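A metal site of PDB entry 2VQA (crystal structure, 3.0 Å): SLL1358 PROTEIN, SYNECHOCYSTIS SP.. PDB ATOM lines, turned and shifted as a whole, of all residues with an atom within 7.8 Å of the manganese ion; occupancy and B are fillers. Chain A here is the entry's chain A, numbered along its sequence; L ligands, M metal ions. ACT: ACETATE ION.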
ATOM      1  N   ILE A 239      25.849 -15.030   8.923  1.00  0.00           N
ATOM      2  CA  ILE A 239      27.291 -15.209   8.970  1.00  0.00           C
ATOM      3  C   ILE A 239      27.898 -14.676  10.266  1.00  0.00           C
ATOM      4  O   ILE A 239      27.618 -13.542  10.663  1.00  0.00           O
ATOM      5  CB  ILE A 239      27.959 -14.452   7.855  1.00  0.00           C
ATOM      6  CG1 ILE A 239      27.388 -14.870   6.500  1.00  0.00           C
ATOM      7  CG2 ILE A 239      29.453 -14.691   7.922  1.00  0.00           C
ATOM      8  CD1 ILE A 239      27.810 -13.960   5.366  1.00  0.00           C
ATOM      9  N   ARG A 247      34.854 -13.804   4.585  1.00  0.00           N
ATOM     10  CA  ARG A 247      34.166 -14.638   3.597  1.00  0.00           C
ATOM     11  C   ARG A 247      34.971 -14.490   2.327  1.00  0.00           C
ATOM     12  O   ARG A 247      35.254 -13.356   1.903  1.00  0.00           O
ATOM     13  CB  ARG A 247      32.746 -14.109   3.348  1.00  0.00           C
ATOM     14  CG  ARG A 247      31.649 -15.122   3.651  1.00  0.00           C
ATOM     15  CD  ARG A 247      30.869 -15.622   2.437  1.00  0.00           C
ATOM     16  NE  ARG A 247      31.641 -16.582   1.669  1.00  0.00           N
ATOM     17  CZ  ARG A 247      31.163 -17.253   0.631  1.00  0.00           C
ATOM     18  NH1 ARG A 247      29.904 -17.093   0.245  1.00  0.00           N
ATOM     19  NH2 ARG A 247      31.941 -18.097  -0.018  1.00  0.00           N
ATOM     20  N   GLN A 248      35.368 -15.593   1.704  1.00  0.00           N
ATOM     21  CA  GLN A 248      36.261 -15.518   0.553  1.00  0.00           C
ATOM     22  C   GLN A 248      35.629 -14.722  -0.582  1.00  0.00           C
ATOM     23  O   GLN A 248      34.428 -14.471  -0.577  1.00  0.00           O
ATOM     24  CB  GLN A 248      36.627 -16.903   0.067  1.00  0.00           C
ATOM     25  CG  GLN A 248      37.475 -17.646   1.031  1.00  0.00           C
ATOM     26  CD  GLN A 248      37.987 -18.937   0.435  1.00  0.00           C
ATOM     27  OE1 GLN A 248      37.898 -19.149  -0.785  1.00  0.00           O
ATOM     28  NE2 GLN A 248      38.523 -19.807   1.290  1.00  0.00           N
ATOM     29  N   HIS A 250      33.812 -14.011  -3.898  1.00  0.00           N
ATOM     30  CA  HIS A 250      32.842 -14.768  -4.675  1.00  0.00           C
ATOM     31  C   HIS A 250      31.871 -13.860  -5.419  1.00  0.00           C
ATOM     32  O   HIS A 250      31.896 -12.631  -5.261  1.00  0.00           O
ATOM     33  CB  HIS A 250      32.069 -15.713  -3.765  1.00  0.00           C
ATOM     34  CG  HIS A 250      31.185 -15.029  -2.767  1.00  0.00           C
ATOM     35  ND1 HIS A 250      31.650 -14.543  -1.570  1.00  0.00           N
ATOM     36  CD2 HIS A 250      29.858 -14.750  -2.800  1.00  0.00           C
ATOM     37  CE1 HIS A 250      30.659 -13.991  -0.900  1.00  0.00           C
ATOM     38  NE2 HIS A 250      29.554 -14.109  -1.627  1.00  0.00           N
ATOM     39  N   TRP A 251      31.020 -14.458  -6.246  1.00  0.00           N
ATOM     40  CA  TRP A 251      29.878 -13.745  -6.813  1.00  0.00           C
ATOM     41  C   TRP A 251      28.673 -14.670  -6.825  1.00  0.00           C
ATOM     42  O   TRP A 251      28.845 -15.886  -6.769  1.00  0.00           O
ATOM     43  CB  TRP A 251      30.165 -13.188  -8.201  1.00  0.00           C
ATOM     44  CG  TRP A 251      30.147 -14.206  -9.282  1.00  0.00           C
ATOM     45  CD1 TRP A 251      29.062 -14.610 -10.022  1.00  0.00           C
ATOM     46  CD2 TRP A 251      31.256 -14.953  -9.771  1.00  0.00           C
ATOM     47  NE1 TRP A 251      29.441 -15.571 -10.929  1.00  0.00           N
ATOM     48  CE2 TRP A 251      30.783 -15.795 -10.795  1.00  0.00           C
ATOM     49  CE3 TRP A 251      32.620 -14.996  -9.438  1.00  0.00           C
ATOM     50  CZ2 TRP A 251      31.606 -16.665 -11.478  1.00  0.00           C
ATOM     51  CZ3 TRP A 251      33.424 -15.856 -10.115  1.00  0.00           C
ATOM     52  CH2 TRP A 251      32.917 -16.684 -11.122  1.00  0.00           C
ATOM     53  N   HIS A 252      27.465 -14.109  -6.865  1.00  0.00           N
ATOM     54  CA  HIS A 252      26.273 -14.933  -7.025  1.00  0.00           C
ATOM     55  C   HIS A 252      25.695 -14.773  -8.428  1.00  0.00           C
ATOM     56  O   HIS A 252      25.305 -13.683  -8.805  1.00  0.00           O
ATOM     57  CB  HIS A 252      25.203 -14.564  -5.997  1.00  0.00           C
ATOM     58  CG  HIS A 252      25.704 -14.527  -4.591  1.00  0.00           C
ATOM     59  ND1 HIS A 252      25.849 -15.654  -3.820  1.00  0.00           N
ATOM     60  CD2 HIS A 252      26.085 -13.484  -3.815  1.00  0.00           C
ATOM     61  CE1 HIS A 252      26.314 -15.313  -2.626  1.00  0.00           C
ATOM     62  NE2 HIS A 252      26.465 -14.006  -2.597  1.00  0.00           N
ATOM     63  N   ASP A 256      20.602 -10.902  -6.190  1.00  0.00           N
ATOM     64  CA  ASP A 256      21.149  -9.767  -5.449  1.00  0.00           C
ATOM     65  C   ASP A 256      21.366 -10.163  -3.966  1.00  0.00           C
ATOM     66  O   ASP A 256      20.773 -11.115  -3.484  1.00  0.00           O
ATOM     67  CB  ASP A 256      20.215  -8.571  -5.578  1.00  0.00           C
ATOM     68  CG  ASP A 256      19.976  -8.166  -7.026  1.00  0.00           C
ATOM     69  OD1 ASP A 256      20.933  -7.818  -7.738  1.00  0.00           O
ATOM     70  OD2 ASP A 256      18.828  -8.173  -7.465  1.00  0.00           O
ATOM     71  N   GLU A 257      22.217  -9.454  -3.242  1.00  0.00           N
ATOM     72  CA  GLU A 257      22.437  -9.757  -1.836  1.00  0.00           C
ATOM     73  C   GLU A 257      22.205  -8.472  -1.046  1.00  0.00           C
ATOM     74  O   GLU A 257      22.831  -7.455  -1.324  1.00  0.00           O
ATOM     75  CB  GLU A 257      23.868 -10.283  -1.605  1.00  0.00           C
ATOM     76  CG  GLU A 257      24.296 -10.512  -0.156  1.00  0.00           C
ATOM     77  CD  GLU A 257      25.640 -11.242  -0.052  1.00  0.00           C
ATOM     78  OE1 GLU A 257      26.005 -11.984  -0.999  1.00  0.00           O
ATOM     79  OE2 GLU A 257      26.348 -11.078   0.964  1.00  0.00           O
ATOM     80  N   GLN A 259      22.215  -6.858   2.826  1.00  0.00           N
ATOM     81  CA  GLN A 259      22.904  -7.142   4.097  1.00  0.00           C
ATOM     82  C   GLN A 259      22.562  -6.216   5.261  1.00  0.00           C
ATOM     83  O   GLN A 259      22.299  -5.028   5.082  1.00  0.00           O
ATOM     84  CB  GLN A 259      24.405  -7.122   3.857  1.00  0.00           C
ATOM     85  CG  GLN A 259      24.792  -7.782   2.564  1.00  0.00           C
ATOM     86  CD  GLN A 259      26.239  -7.579   2.229  1.00  0.00           C
ATOM     87  OE1 GLN A 259      26.816  -6.551   2.546  1.00  0.00           O
ATOM     88  NE2 GLN A 259      26.852  -8.579   1.584  1.00  0.00           N
ATOM     89  N   LEU A 268      33.280  -4.340   3.694  1.00  0.00           N
ATOM     90  CA  LEU A 268      32.769  -4.975   2.487  1.00  0.00           C
ATOM     91  C   LEU A 268      33.481  -4.407   1.274  1.00  0.00           C
ATOM     92  O   LEU A 268      33.729  -3.217   1.201  1.00  0.00           O
ATOM     93  CB  LEU A 268      31.260  -4.748   2.388  1.00  0.00           C
ATOM     94  CG  LEU A 268      30.591  -4.867   1.025  1.00  0.00           C
ATOM     95  CD1 LEU A 268      30.377  -6.323   0.716  1.00  0.00           C
ATOM     96  CD2 LEU A 268      29.285  -4.123   1.017  1.00  0.00           C
ATOM     97  N   VAL A 290      24.767  -5.979  -2.594  1.00  0.00           N
ATOM     98  CA  VAL A 290      25.610  -6.392  -3.716  1.00  0.00           C
ATOM     99  C   VAL A 290      24.743  -6.828  -4.913  1.00  0.00           C
ATOM    100  O   VAL A 290      24.048  -7.838  -4.825  1.00  0.00           O
ATOM    101  CB  VAL A 290      26.545  -7.551  -3.317  1.00  0.00           C
ATOM    102  CG1 VAL A 290      27.524  -7.848  -4.435  1.00  0.00           C
ATOM    103  CG2 VAL A 290      27.278  -7.240  -2.018  1.00  0.00           C
ATOM    104  N   TYR A 294      28.075  -9.204  -9.181  1.00  0.00           N
ATOM    105  CA  TYR A 294      29.248  -8.429  -8.763  1.00  0.00           C
ATOM    106  C   TYR A 294      30.123  -9.275  -7.865  1.00  0.00           C
ATOM    107  O   TYR A 294      29.628 -10.047  -7.035  1.00  0.00           O
ATOM    108  CB  TYR A 294      28.850  -7.137  -8.023  1.00  0.00           C
ATOM    109  CG  TYR A 294      28.350  -5.977  -8.892  1.00  0.00           C
ATOM    110  CD1 TYR A 294      28.451  -4.665  -8.449  1.00  0.00           C
ATOM    111  CD2 TYR A 294      27.776  -6.209 -10.147  1.00  0.00           C
ATOM    112  CE1 TYR A 294      27.985  -3.607  -9.225  1.00  0.00           C
ATOM    113  CE2 TYR A 294      27.310  -5.151 -10.923  1.00  0.00           C
ATOM    114  CZ  TYR A 294      27.413  -3.859 -10.470  1.00  0.00           C
ATOM    115  OH  TYR A 294      26.958  -2.809 -11.246  1.00  0.00           O
ATOM    116  N   HIS A 296      32.598  -9.883  -4.782  1.00  0.00           N
ATOM    117  CA  HIS A 296      32.608  -9.289  -3.458  1.00  0.00           C
ATOM    118  C   HIS A 296      33.201 -10.218  -2.395  1.00  0.00           C
ATOM    119  O   HIS A 296      33.445 -11.399  -2.640  1.00  0.00           O
ATOM    120  CB  HIS A 296      31.205  -8.799  -3.077  1.00  0.00           C
ATOM    121  CG  HIS A 296      30.173  -9.885  -2.965  1.00  0.00           C
ATOM    122  ND1 HIS A 296      29.773 -10.644  -4.038  1.00  0.00           N
ATOM    123  CD2 HIS A 296      29.442 -10.300  -1.908  1.00  0.00           C
ATOM    124  CE1 HIS A 296      28.842 -11.504  -3.639  1.00  0.00           C
ATOM    125  NE2 HIS A 296      28.626 -11.320  -2.352  1.00  0.00           N
ATOM    126  N   ALA A 297      33.450  -9.635  -1.226  1.00  0.00           N
ATOM    127  CA  ALA A 297      34.060 -10.330  -0.102  1.00  0.00           C
ATOM    128  C   ALA A 297      33.828  -9.465   1.106  1.00  0.00           C
ATOM    129  O   ALA A 297      33.703  -8.239   0.976  1.00  0.00           O
ATOM    130  CB  ALA A 297      35.557 -10.531  -0.325  1.00  0.00           C
ATOM    131  N   ILE A 298      33.759 -10.078   2.279  1.00  0.00           N
ATOM    132  CA  ILE A 298      33.573  -9.317   3.497  1.00  0.00           C
ATOM    133  C   ILE A 298      34.535  -9.772   4.594  1.00  0.00           C
ATOM    134  O   ILE A 298      34.718 -10.968   4.839  1.00  0.00           O
ATOM    135  CB  ILE A 298      32.081  -9.280   3.962  1.00  0.00           C
ATOM    136  CG1 ILE A 298      31.742 -10.406   4.924  1.00  0.00           C
ATOM    137  CG2 ILE A 298      31.138  -9.388   2.775  1.00  0.00           C
ATOM    138  CD1 ILE A 298      30.288 -10.857   4.753  1.00  0.00           C
ATOM    139  N   VAL A 310      22.148 -11.801   5.766  1.00  0.00           N
ATOM    140  CA  VAL A 310      22.004 -11.443   4.356  1.00  0.00           C
ATOM    141  C   VAL A 310      20.812 -12.165   3.747  1.00  0.00           C
ATOM    142  O   VAL A 310      20.429 -13.241   4.190  1.00  0.00           O
ATOM    143  CB  VAL A 310      23.252 -11.788   3.547  1.00  0.00           C
ATOM    144  CG1 VAL A 310      24.420 -10.923   3.979  1.00  0.00           C
ATOM    145  CG2 VAL A 310      23.581 -13.248   3.702  1.00  0.00           C
ATOM    146  N   PHE A 312      18.780 -13.033  -0.139  1.00  0.00           N
ATOM    147  CA  PHE A 312      18.862 -13.055  -1.600  1.00  0.00           C
ATOM    148  C   PHE A 312      17.489 -13.148  -2.232  1.00  0.00           C
ATOM    149  O   PHE A 312      16.634 -13.883  -1.743  1.00  0.00           O
ATOM    150  CB  PHE A 312      19.669 -14.254  -2.080  1.00  0.00           C
ATOM    151  CG  PHE A 312      21.001 -14.384  -1.427  1.00  0.00           C
ATOM    152  CD1 PHE A 312      22.115 -13.831  -2.005  1.00  0.00           C
ATOM    153  CD2 PHE A 312      21.131 -15.057  -0.228  1.00  0.00           C
ATOM    154  CE1 PHE A 312      23.342 -13.954  -1.406  1.00  0.00           C
ATOM    155  CE2 PHE A 312      22.356 -15.171   0.381  1.00  0.00           C
ATOM    156  CZ  PHE A 312      23.461 -14.619  -0.208  1.00  0.00           C
ATOM    157  N   TYR A 317      20.051 -20.773  -3.579  1.00  0.00           N
ATOM    158  CA  TYR A 317      21.311 -20.140  -3.252  1.00  0.00           C
ATOM    159  C   TYR A 317      22.440 -20.621  -4.151  1.00  0.00           C
ATOM    160  O   TYR A 317      22.746 -21.806  -4.199  1.00  0.00           O
ATOM    161  CB  TYR A 317      21.676 -20.407  -1.803  1.00  0.00           C
ATOM    162  CG  TYR A 317      23.052 -19.925  -1.444  1.00  0.00           C
ATOM    163  CD1 TYR A 317      23.282 -18.570  -1.164  1.00  0.00           C
ATOM    164  CD2 TYR A 317      24.121 -20.810  -1.393  1.00  0.00           C
ATOM    165  CE1 TYR A 317      24.554 -18.125  -0.826  1.00  0.00           C
ATOM    166  CE2 TYR A 317      25.392 -20.368  -1.073  1.00  0.00           C
ATOM    167  CZ  TYR A 317      25.599 -19.034  -0.799  1.00  0.00           C
ATOM    168  OH  TYR A 317      26.873 -18.636  -0.476  1.00  0.00           O
ATOM    169  N   GLN A 318      23.057 -19.679  -4.862  1.00  0.00           N
ATOM    170  CA  GLN A 318      24.139 -19.988  -5.796  1.00  0.00           C
ATOM    171  C   GLN A 318      25.359 -19.093  -5.556  1.00  0.00           C
ATOM    172  O   GLN A 318      25.251 -17.854  -5.537  1.00  0.00           O
ATOM    173  CB  GLN A 318      23.644 -19.851  -7.236  1.00  0.00           C
ATOM    174  CG  GLN A 318      22.800 -20.997  -7.707  1.00  0.00           C
ATOM    175  CD  GLN A 318      22.294 -20.811  -9.126  1.00  0.00           C
ATOM    176  OE1 GLN A 318      22.932 -20.154  -9.950  1.00  0.00           O
ATOM    177  NE2 GLN A 318      21.129 -21.382  -9.418  1.00  0.00           N
ATOM    178  N   SER A 319      26.515 -19.737  -5.373  1.00  0.00           N
ATOM    179  CA  SER A 319      27.769 -19.034  -5.094  1.00  0.00           C
ATOM    180  C   SER A 319      28.858 -19.671  -5.927  1.00  0.00           C
ATOM    181  O   SER A 319      28.878 -20.877  -6.087  1.00  0.00           O
ATOM    182  CB  SER A 319      28.127 -19.174  -3.598  1.00  0.00           C
ATOM    183  OG  SER A 319      29.382 -18.583  -3.263  1.00  0.00           O
ATOM    184  N   ASP A 321      32.893 -19.333  -5.532  1.00  0.00           N
ATOM    185  CA  ASP A 321      34.021 -18.714  -4.823  1.00  0.00           C
ATOM    186  C   ASP A 321      35.230 -18.638  -5.719  1.00  0.00           C
ATOM    187  O   ASP A 321      35.453 -19.517  -6.554  1.00  0.00           O
ATOM    188  CB  ASP A 321      34.418 -19.498  -3.563  1.00  0.00           C
ATOM    189  CG  ASP A 321      33.356 -19.473  -2.477  1.00  0.00           C
ATOM    190  OD1 ASP A 321      33.317 -20.428  -1.668  1.00  0.00           O
ATOM    191  OD2 ASP A 321      32.568 -18.505  -2.427  1.00  0.00           O
HETATM  192  C   ACT L   1      27.166 -15.423   1.215  1.00  0.00           C
HETATM  193  O   ACT L   1      27.623 -14.318   0.890  1.00  0.00           O
HETATM  194  OXT ACT L   1      27.001 -16.242   0.295  1.00  0.00           O
HETATM  195  CH3 ACT L   1      26.817 -15.774   2.622  1.00  0.00           C
HETATM  196 MN    MN M   1      27.735 -12.995  -0.940  1.00  0.00          MN
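ND1 of His 296 sits at hydrogen-bond distance from O of Tyr 294, 3.1 Å away.
The backbone carbonyl oxygen of Gln 248 sits at hydrogen-bond distance from a ring nitrogen (ND1) of His 250.
The backbone carbonyl oxygen (O) of Gln 318 lies within hydrogen-bond range of a ring nitrogen (ND1) of His 252.
The backbone carbonyl oxygen (O) of Glu 257 sits at hydrogen-bond distance from the backbone NH (N) of Val 290 (2.7 Å).
OE2 of Glu 257 sits at hydrogen-bond distance from NE2 of Gln 259, 2.6 Å away.
Four residues have an atom within 4 Å of the manganese ion: His 250, His 252, Glu 257 and His 296.
The nearest printed residue that does not touch the manganese ion is Phe 312 (4.5 Å).
The manganese ion is bound by OE1 of Glu 257 (2.0 Å).
The manganese ion is bound by NE2 of His 250 (2.2 Å).
O of the ligand is bound to the manganese ion, 2.3 Å away.
A ring nitrogen (NE2) of His 252 is bound to the manganese ion.
A ring nitrogen (NE2) of His 296 is bound to the manganese ion.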
